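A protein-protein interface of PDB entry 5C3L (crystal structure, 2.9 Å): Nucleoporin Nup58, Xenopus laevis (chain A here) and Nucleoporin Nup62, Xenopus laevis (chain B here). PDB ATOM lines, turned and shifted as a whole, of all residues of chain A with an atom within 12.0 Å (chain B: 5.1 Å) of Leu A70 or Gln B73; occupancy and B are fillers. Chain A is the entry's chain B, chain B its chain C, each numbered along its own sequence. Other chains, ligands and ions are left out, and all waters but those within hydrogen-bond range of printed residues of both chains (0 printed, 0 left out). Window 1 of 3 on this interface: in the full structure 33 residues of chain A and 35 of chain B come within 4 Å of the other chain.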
ATOM      1  N   GLN A  61     -33.795   5.535  -7.099  1.00  0.00           N
ATOM      2  CA  GLN A  61     -32.476   5.611  -6.467  1.00  0.00           C
ATOM      3  C   GLN A  61     -31.781   4.247  -6.371  1.00  0.00           C
ATOM      4  O   GLN A  61     -30.569   4.148  -6.575  1.00  0.00           O
ATOM      5  CB  GLN A  61     -32.582   6.214  -5.062  1.00  0.00           C
ATOM      6  CG  GLN A  61     -31.230   6.379  -4.349  1.00  0.00           C
ATOM      7  CD  GLN A  61     -30.265   7.267  -5.120  1.00  0.00           C
ATOM      8  OE1 GLN A  61     -30.686   8.121  -5.897  1.00  0.00           O
ATOM      9  NE2 GLN A  61     -28.967   7.063  -4.919  1.00  0.00           N
ATOM     10  N   LEU A  62     -32.541   3.209  -6.030  1.00  0.00           N
ATOM     11  CA  LEU A  62     -32.013   1.851  -5.971  1.00  0.00           C
ATOM     12  C   LEU A  62     -31.642   1.347  -7.368  1.00  0.00           C
ATOM     13  O   LEU A  62     -30.568   0.764  -7.576  1.00  0.00           O
ATOM     14  CB  LEU A  62     -33.035   0.912  -5.333  1.00  0.00           C
ATOM     15  CG  LEU A  62     -33.418   1.196  -3.882  1.00  0.00           C
ATOM     16  CD1 LEU A  62     -34.231   0.041  -3.356  1.00  0.00           C
ATOM     17  CD2 LEU A  62     -32.209   1.452  -2.978  1.00  0.00           C
ATOM     18  N   LEU A  63     -32.535   1.568  -8.323  1.00  0.00           N
ATOM     19  CA  LEU A  63     -32.297   1.138  -9.687  1.00  0.00           C
ATOM     20  C   LEU A  63     -31.030   1.770 -10.238  1.00  0.00           C
ATOM     21  O   LEU A  63     -30.263   1.140 -10.965  1.00  0.00           O
ATOM     22  CB  LEU A  63     -33.480   1.511 -10.569  1.00  0.00           C
ATOM     23  CG  LEU A  63     -33.561   0.707 -11.862  1.00  0.00           C
ATOM     24  CD1 LEU A  63     -34.235  -0.619 -11.564  1.00  0.00           C
ATOM     25  CD2 LEU A  63     -34.286   1.483 -12.965  1.00  0.00           C
ATOM     26  N   SER A  64     -30.822   3.031  -9.887  1.00  0.00           N
ATOM     27  CA  SER A  64     -29.717   3.805 -10.432  1.00  0.00           C
ATOM     28  C   SER A  64     -28.376   3.291  -9.936  1.00  0.00           C
ATOM     29  O   SER A  64     -27.447   3.113 -10.726  1.00  0.00           O
ATOM     30  CB  SER A  64     -29.885   5.275 -10.071  1.00  0.00           C
ATOM     31  OG  SER A  64     -31.075   5.786 -10.639  1.00  0.00           O
ATOM     32  N   VAL A  65     -28.268   3.042  -8.633  1.00  0.00           N
ATOM     33  CA  VAL A  65     -27.029   2.501  -8.108  1.00  0.00           C
ATOM     34  C   VAL A  65     -26.782   1.130  -8.746  1.00  0.00           C
ATOM     35  O   VAL A  65     -25.650   0.816  -9.128  1.00  0.00           O
ATOM     36  CB  VAL A  65     -27.039   2.404  -6.566  1.00  0.00           C
ATOM     37  CG1 VAL A  65     -27.217   3.794  -5.974  1.00  0.00           C
ATOM     38  CG2 VAL A  65     -28.123   1.475  -6.081  1.00  0.00           C
ATOM     39  N   ALA A  66     -27.845   0.344  -8.914  1.00  0.00           N
ATOM     40  CA  ALA A  66     -27.710  -0.999  -9.467  1.00  0.00           C
ATOM     41  C   ALA A  66     -27.204  -0.931 -10.896  1.00  0.00           C
ATOM     42  O   ALA A  66     -26.228  -1.609 -11.249  1.00  0.00           O
ATOM     43  CB  ALA A  66     -29.023  -1.738  -9.417  1.00  0.00           C
ATOM     44  N   SER A  67     -27.860  -0.109 -11.711  1.00  0.00           N
ATOM     45  CA  SER A  67     -27.497  -0.012 -13.115  1.00  0.00           C
ATOM     46  C   SER A  67     -26.082   0.573 -13.235  1.00  0.00           C
ATOM     47  O   SER A  67     -25.331   0.180 -14.128  1.00  0.00           O
ATOM     48  CB  SER A  67     -28.522   0.822 -13.892  1.00  0.00           C
ATOM     49  OG  SER A  67     -28.195   2.194 -13.859  1.00  0.00           O
ATOM     50  N   SER A  68     -25.701   1.479 -12.336  1.00  0.00           N
ATOM     51  CA  SER A  68     -24.318   1.974 -12.308  1.00  0.00           C
ATOM     52  C   SER A  68     -23.295   0.837 -12.133  1.00  0.00           C
ATOM     53  O   SER A  68     -22.352   0.715 -12.922  1.00  0.00           O
ATOM     54  CB  SER A  68     -24.127   2.994 -11.188  1.00  0.00           C
ATOM     55  OG  SER A  68     -24.867   4.156 -11.458  1.00  0.00           O
ATOM     56  N   GLY A  69     -23.482   0.027 -11.093  1.00  0.00           N
ATOM     57  CA  GLY A  69     -22.646  -1.135 -10.853  1.00  0.00           C
ATOM     58  C   GLY A  69     -22.722  -2.157 -11.976  1.00  0.00           C
ATOM     59  O   GLY A  69     -21.771  -2.901 -12.219  1.00  0.00           O
ATOM     60  N   LEU A  70     -23.851  -2.192 -12.675  1.00  0.00           N
ATOM     61  CA  LEU A  70     -23.992  -3.099 -13.810  1.00  0.00           C
ATOM     62  C   LEU A  70     -23.039  -2.702 -14.919  1.00  0.00           C
ATOM     63  O   LEU A  70     -22.507  -3.555 -15.608  1.00  0.00           O
ATOM     64  CB  LEU A  70     -25.431  -3.119 -14.344  1.00  0.00           C
ATOM     65  CG  LEU A  70     -25.742  -4.218 -15.374  1.00  0.00           C
ATOM     66  CD1 LEU A  70     -27.163  -4.724 -15.189  1.00  0.00           C
ATOM     67  CD2 LEU A  70     -25.540  -3.743 -16.804  1.00  0.00           C
ATOM     68  N   GLN A  71     -22.825  -1.407 -15.104  1.00  0.00           N
ATOM     69  CA  GLN A  71     -21.951  -0.959 -16.181  1.00  0.00           C
ATOM     70  C   GLN A  71     -20.515  -1.137 -15.759  1.00  0.00           C
ATOM     71  O   GLN A  71     -19.643  -1.393 -16.582  1.00  0.00           O
ATOM     72  CB  GLN A  71     -22.213   0.500 -16.550  1.00  0.00           C
ATOM     73  CG  GLN A  71     -22.337   0.716 -18.055  1.00  0.00           C
ATOM     74  CD  GLN A  71     -23.493  -0.077 -18.646  1.00  0.00           C
ATOM     75  OE1 GLN A  71     -24.574  -0.147 -18.051  1.00  0.00           O
ATOM     76  NE2 GLN A  71     -23.269  -0.691 -19.809  1.00  0.00           N
ATOM     77  N   ARG A  72     -20.273  -1.009 -14.462  1.00  0.00           N
ATOM     78  CA  ARG A  72     -18.928  -1.133 -13.931  1.00  0.00           C
ATOM     79  C   ARG A  72     -18.361  -2.534 -14.199  1.00  0.00           C
ATOM     80  O   ARG A  72     -17.227  -2.685 -14.688  1.00  0.00           O
ATOM     81  CB  ARG A  72     -18.930  -0.819 -12.438  1.00  0.00           C
ATOM     82  CG  ARG A  72     -18.330   0.533 -12.110  1.00  0.00           C
ATOM     83  CD  ARG A  72     -18.364   0.807 -10.625  1.00  0.00           C
ATOM     84  NE  ARG A  72     -19.487   1.658 -10.256  1.00  0.00           N
ATOM     85  CZ  ARG A  72     -20.454   1.331  -9.402  1.00  0.00           C
ATOM     86  NH1 ARG A  72     -20.465   0.157  -8.791  1.00  0.00           N
ATOM     87  NH2 ARG A  72     -21.423   2.199  -9.148  1.00  0.00           N
ATOM     88  N   ASN A  73     -19.156  -3.562 -13.924  1.00  0.00           N
ATOM     89  CA  ASN A  73     -18.647  -4.910 -14.024  1.00  0.00           C
ATOM     90  C   ASN A  73     -19.022  -5.562 -15.368  1.00  0.00           C
ATOM     91  O   ASN A  73     -18.608  -6.684 -15.653  1.00  0.00           O
ATOM     92  CB  ASN A  73     -19.131  -5.731 -12.813  1.00  0.00           C
ATOM     93  CG  ASN A  73     -20.622  -5.765 -12.691  1.00  0.00           C
ATOM     94  OD1 ASN A  73     -21.325  -5.657 -13.679  1.00  0.00           O
ATOM     95  ND2 ASN A  73     -21.118  -5.926 -11.472  1.00  0.00           N
ATOM     96  N   ALA A  74     -19.779  -4.847 -16.201  1.00  0.00           N
ATOM     97  CA  ALA A  74     -19.952  -5.233 -17.606  1.00  0.00           C
ATOM     98  C   ALA A  74     -18.641  -4.975 -18.340  1.00  0.00           C
ATOM     99  O   ALA A  74     -18.246  -5.744 -19.211  1.00  0.00           O
ATOM    100  CB  ALA A  74     -21.080  -4.467 -18.251  1.00  0.00           C
ATOM    101  N   LEU A  75     -17.969  -3.888 -17.967  1.00  0.00           N
ATOM    102  CA  LEU A  75     -16.599  -3.624 -18.406  1.00  0.00           C
ATOM    103  C   LEU A  75     -15.649  -4.715 -17.931  1.00  0.00           C
ATOM    104  O   LEU A  75     -14.769  -5.154 -18.666  1.00  0.00           O
ATOM    105  CB  LEU A  75     -16.107  -2.273 -17.880  1.00  0.00           C
ATOM    106  CG  LEU A  75     -16.692  -0.994 -18.476  1.00  0.00           C
ATOM    107  CD1 LEU A  75     -15.923   0.212 -17.965  1.00  0.00           C
ATOM    108  CD2 LEU A  75     -16.697  -1.032 -19.996  1.00  0.00           C
ATOM    109  N   ALA A  76     -15.827  -5.127 -16.683  1.00  0.00           N
ATOM    110  CA  ALA A  76     -15.010  -6.170 -16.075  1.00  0.00           C
ATOM    111  C   ALA A  76     -15.159  -7.473 -16.842  1.00  0.00           C
ATOM    112  O   ALA A  76     -14.235  -8.284 -16.900  1.00  0.00           O
ATOM    113  CB  ALA A  76     -15.411  -6.369 -14.622  1.00  0.00           C
ATOM    114  N   ILE A  77     -16.329  -7.658 -17.440  1.00  0.00           N
ATOM    115  CA  ILE A  77     -16.683  -8.911 -18.079  1.00  0.00           C
ATOM    116  C   ILE A  77     -16.171  -8.962 -19.510  1.00  0.00           C
ATOM    117  O   ILE A  77     -15.808 -10.018 -20.008  1.00  0.00           O
ATOM    118  CB  ILE A  77     -18.218  -9.117 -18.037  1.00  0.00           C
ATOM    119  CG1 ILE A  77     -18.607  -9.676 -16.668  1.00  0.00           C
ATOM    120  CG2 ILE A  77     -18.701 -10.052 -19.156  1.00  0.00           C
ATOM    121  CD1 ILE A  77     -20.081  -9.727 -16.393  1.00  0.00           C
ATOM    122  N   ASP A  78     -16.127  -7.829 -20.181  1.00  0.00           N
ATOM    123  CA  ASP A  78     -15.656  -7.853 -21.545  1.00  0.00           C
ATOM    124  C   ASP A  78     -14.151  -8.003 -21.513  1.00  0.00           C
ATOM    125  O   ASP A  78     -13.569  -8.681 -22.355  1.00  0.00           O
ATOM    126  CB  ASP A  78     -16.075  -6.597 -22.311  1.00  0.00           C
ATOM    127  CG  ASP A  78     -16.348  -6.889 -23.769  1.00  0.00           C
ATOM    128  OD1 ASP A  78     -17.345  -7.603 -24.040  1.00  0.00           O
ATOM    129  OD2 ASP A  78     -15.568  -6.430 -24.637  1.00  0.00           O
ATOM    130  N   LYS A  79     -13.524  -7.382 -20.523  1.00  0.00           N
ATOM    131  CA  LYS A  79     -12.079  -7.456 -20.389  1.00  0.00           C
ATOM    132  C   LYS A  79     -11.695  -8.911 -20.132  1.00  0.00           C
ATOM    133  O   LYS A  79     -10.711  -9.416 -20.654  1.00  0.00           O
ATOM    134  CB  LYS A  79     -11.601  -6.548 -19.257  1.00  0.00           C
ATOM    135  CG  LYS A  79     -10.108  -6.322 -19.239  1.00  0.00           C
ATOM    136  CD  LYS A  79      -9.610  -5.996 -17.837  1.00  0.00           C
ATOM    137  CE  LYS A  79      -8.091  -6.124 -17.744  1.00  0.00           C
ATOM    138  NZ  LYS A  79      -7.567  -6.056 -16.346  1.00  0.00           N
ATOM    139  N   VAL B  69     -32.976  -2.639 -17.926  1.00  0.00           N
ATOM    140  CA  VAL B  69     -31.900  -3.090 -17.068  1.00  0.00           C
ATOM    141  C   VAL B  69     -31.994  -4.604 -16.857  1.00  0.00           C
ATOM    142  O   VAL B  69     -30.967  -5.283 -16.714  1.00  0.00           O
ATOM    143  CB  VAL B  69     -31.930  -2.344 -15.710  1.00  0.00           C
ATOM    144  CG1 VAL B  69     -30.877  -2.885 -14.762  1.00  0.00           C
ATOM    145  CG2 VAL B  69     -31.697  -0.865 -15.935  1.00  0.00           C
ATOM    146  N   LYS B  70     -33.216  -5.133 -16.835  1.00  0.00           N
ATOM    147  CA  LYS B  70     -33.405  -6.580 -16.788  1.00  0.00           C
ATOM    148  C   LYS B  70     -32.694  -7.240 -17.966  1.00  0.00           C
ATOM    149  O   LYS B  70     -31.991  -8.239 -17.801  1.00  0.00           O
ATOM    150  CB  LYS B  70     -34.881  -6.939 -16.818  1.00  0.00           C
ATOM    151  CG  LYS B  70     -35.490  -7.122 -15.475  1.00  0.00           C
ATOM    152  CD  LYS B  70     -36.974  -7.335 -15.619  1.00  0.00           C
ATOM    153  CE  LYS B  70     -37.641  -7.501 -14.274  1.00  0.00           C
ATOM    154  NZ  LYS B  70     -39.115  -7.512 -14.412  1.00  0.00           N
ATOM    155  N   LEU B  71     -32.904  -6.669 -19.152  1.00  0.00           N
ATOM    156  CA  LEU B  71     -32.294  -7.144 -20.390  1.00  0.00           C
ATOM    157  C   LEU B  71     -30.776  -7.156 -20.312  1.00  0.00           C
ATOM    158  O   LEU B  71     -30.131  -8.153 -20.635  1.00  0.00           O
ATOM    159  CB  LEU B  71     -32.715  -6.259 -21.559  1.00  0.00           C
ATOM    160  CG  LEU B  71     -33.351  -6.993 -22.733  1.00  0.00           C
ATOM    161  CD1 LEU B  71     -34.834  -7.185 -22.469  1.00  0.00           C
ATOM    162  CD2 LEU B  71     -33.100  -6.254 -24.051  1.00  0.00           C
ATOM    163  N   ASP B  72     -30.215  -6.022 -19.902  1.00  0.00           N
ATOM    164  CA  ASP B  72     -28.774  -5.869 -19.789  1.00  0.00           C
ATOM    165  C   ASP B  72     -28.218  -6.904 -18.814  1.00  0.00           C
ATOM    166  O   ASP B  72     -27.138  -7.458 -19.034  1.00  0.00           O
ATOM    167  CB  ASP B  72     -28.412  -4.452 -19.323  1.00  0.00           C
ATOM    168  CG  ASP B  72     -28.824  -3.375 -20.317  1.00  0.00           C
ATOM    169  OD1 ASP B  72     -29.243  -3.706 -21.448  1.00  0.00           O
ATOM    170  OD2 ASP B  72     -28.716  -2.184 -19.963  1.00  0.00           O
ATOM    171  N   GLN B  73     -28.970  -7.171 -17.748  1.00  0.00           N
ATOM    172  CA  GLN B  73     -28.557  -8.150 -16.753  1.00  0.00           C
ATOM    173  C   GLN B  73     -28.469  -9.526 -17.381  1.00  0.00           C
ATOM    174  O   GLN B  73     -27.474 -10.233 -17.214  1.00  0.00           O
ATOM    175  CB  GLN B  73     -29.522  -8.185 -15.576  1.00  0.00           C
ATOM    176  CG  GLN B  73     -29.103  -9.135 -14.458  1.00  0.00           C
ATOM    177  CD  GLN B  73     -27.868  -8.662 -13.719  1.00  0.00           C
ATOM    178  OE1 GLN B  73     -27.617  -7.464 -13.614  1.00  0.00           O
ATOM    179  NE2 GLN B  73     -27.092  -9.602 -13.198  1.00  0.00           N
ATOM    180  N   LYS B  74     -29.519  -9.910 -18.093  1.00  0.00           N
ATOM    181  CA  LYS B  74     -29.547 -11.202 -18.757  1.00  0.00           C
ATOM    182  C   LYS B  74     -28.445 -11.317 -19.817  1.00  0.00           C
ATOM    183  O   LYS B  74     -27.920 -12.402 -20.052  1.00  0.00           O
ATOM    184  CB  LYS B  74     -30.916 -11.445 -19.390  1.00  0.00           C
ATOM    185  CG  LYS B  74     -32.004 -11.737 -18.372  1.00  0.00           C
ATOM    186  CD  LYS B  74     -33.247 -12.349 -19.006  1.00  0.00           C
ATOM    187  CE  LYS B  74     -32.945 -13.726 -19.587  1.00  0.00           C
ATOM    188  NZ  LYS B  74     -34.173 -14.517 -19.867  1.00  0.00           N
ATOM    189  N   ARG B  75     -28.081 -10.210 -20.452  1.00  0.00           N
ATOM    190  CA  ARG B  75     -26.974 -10.241 -21.397  1.00  0.00           C
ATOM    191  C   ARG B  75     -25.673 -10.588 -20.674  1.00  0.00           C
ATOM    192  O   ARG B  75     -24.862 -11.368 -21.161  1.00  0.00           O
ATOM    193  CB  ARG B  75     -26.836  -8.904 -22.111  1.00  0.00           C
ATOM    194  CG  ARG B  75     -25.788  -8.925 -23.213  1.00  0.00           C
ATOM    195  CD  ARG B  75     -24.909  -7.690 -23.157  1.00  0.00           C
ATOM    196  NE  ARG B  75     -23.680  -7.842 -23.938  1.00  0.00           N
ATOM    197  CZ  ARG B  75     -22.614  -7.058 -23.806  1.00  0.00           C
ATOM    198  NH1 ARG B  75     -22.617  -6.062 -22.921  1.00  0.00           N
ATOM    199  NH2 ARG B  75     -21.540  -7.272 -24.551  1.00  0.00           N
ATOM    200  N   LEU B  76     -25.485  -9.990 -19.502  1.00  0.00           N
ATOM    201  CA  LEU B  76     -24.314 -10.250 -18.677  1.00  0.00           C
ATOM    202  C   LEU B  76     -24.301 -11.711 -18.244  1.00  0.00           C
ATOM    203  O   LEU B  76     -23.262 -12.360 -18.281  1.00  0.00           O
ATOM    204  CB  LEU B  76     -24.306  -9.312 -17.467  1.00  0.00           C
ATOM    205  CG  LEU B  76     -23.305  -8.152 -17.507  1.00  0.00           C
ATOM    206  CD1 LEU B  76     -23.253  -7.474 -18.879  1.00  0.00           C
ATOM    207  CD2 LEU B  76     -23.637  -7.141 -16.416  1.00  0.00           C
ATOM    208  N   ASP B  77     -25.462 -12.235 -17.858  1.00  0.00           N
ATOM    209  CA  ASP B  77     -25.573 -13.636 -17.467  1.00  0.00           C
ATOM    210  C   ASP B  77     -25.108 -14.560 -18.599  1.00  0.00           C
ATOM    211  O   ASP B  77     -24.417 -15.546 -18.362  1.00  0.00           O
ATOM    212  CB  ASP B  77     -27.015 -13.971 -17.068  1.00  0.00           C
ATOM    213  CG  ASP B  77     -27.446 -13.297 -15.774  1.00  0.00           C
ATOM    214  OD1 ASP B  77     -26.578 -12.969 -14.936  1.00  0.00           O
ATOM    215  OD2 ASP B  77     -28.665 -13.105 -15.590  1.00  0.00           O
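The side-chain amide oxygen (OD1) of Asn A73 sits close to the backbone carbonyl oxygen (O) of Gly A69.
The backbone carbonyl oxygen (O) of Leu A70 lies close to the side-chain amide oxygen (OD1) of Asn A73, 3.1 Å away.
Among the printed residues, merely in contact across the chains: Leu A70 with Gln B73 (3.2 Å), Leu A70 with Leu B76 (3.7 Å), Ile A77 with Leu B76 (3.8 Å), Ala A74 with Leu B76 (3.8 Å), Asn A73 with Leu B76 (3.9 Å) and Leu A70 with Asp B72 (3.9 Å).
Leu A70 touches just these residues of chain B: Asp B72, Gln B73 and Leu B76.
Of the printed residues of chain B, Asn A73 touches Leu B76.
Of the printed residues of chain B, Ala A74 touches Leu B76 (3.8 Å).
Printed residues of chain B within 4 Å of Ile A77: Leu B76 (3.8 Å).
No residue of chain A comes within 4 Å of Val B69.
No residue of chain A comes within 4 Å of Leu B71.
Asp B72 touches one residue of chain A.
Of chain A, only Leu A70 comes within 4 Å of Gln B73.
Leu B76 touches just these residues of chain A: Leu A70 (3.7 Å), Asn A73 (3.9 Å), Ala A74 (3.8 Å) and Ile A77 (3.8 Å).
The nearest residue of chain A that does not touch Gln B73 is Ala A66 (6.5 Å).
The nearest printed residue of chain B that does not touch Ala A74 is Arg B75 (5.2 Å).
Of the 19 printed residues of chain A, 4 touch a printed residue of chain B.
Among the printed residues, 6 pairs touch across the chains.
Among the printed residues, no Asp or Glu carboxylate lies within 4 Å of a Lys or Arg side-chain nitrogen of the other chain.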
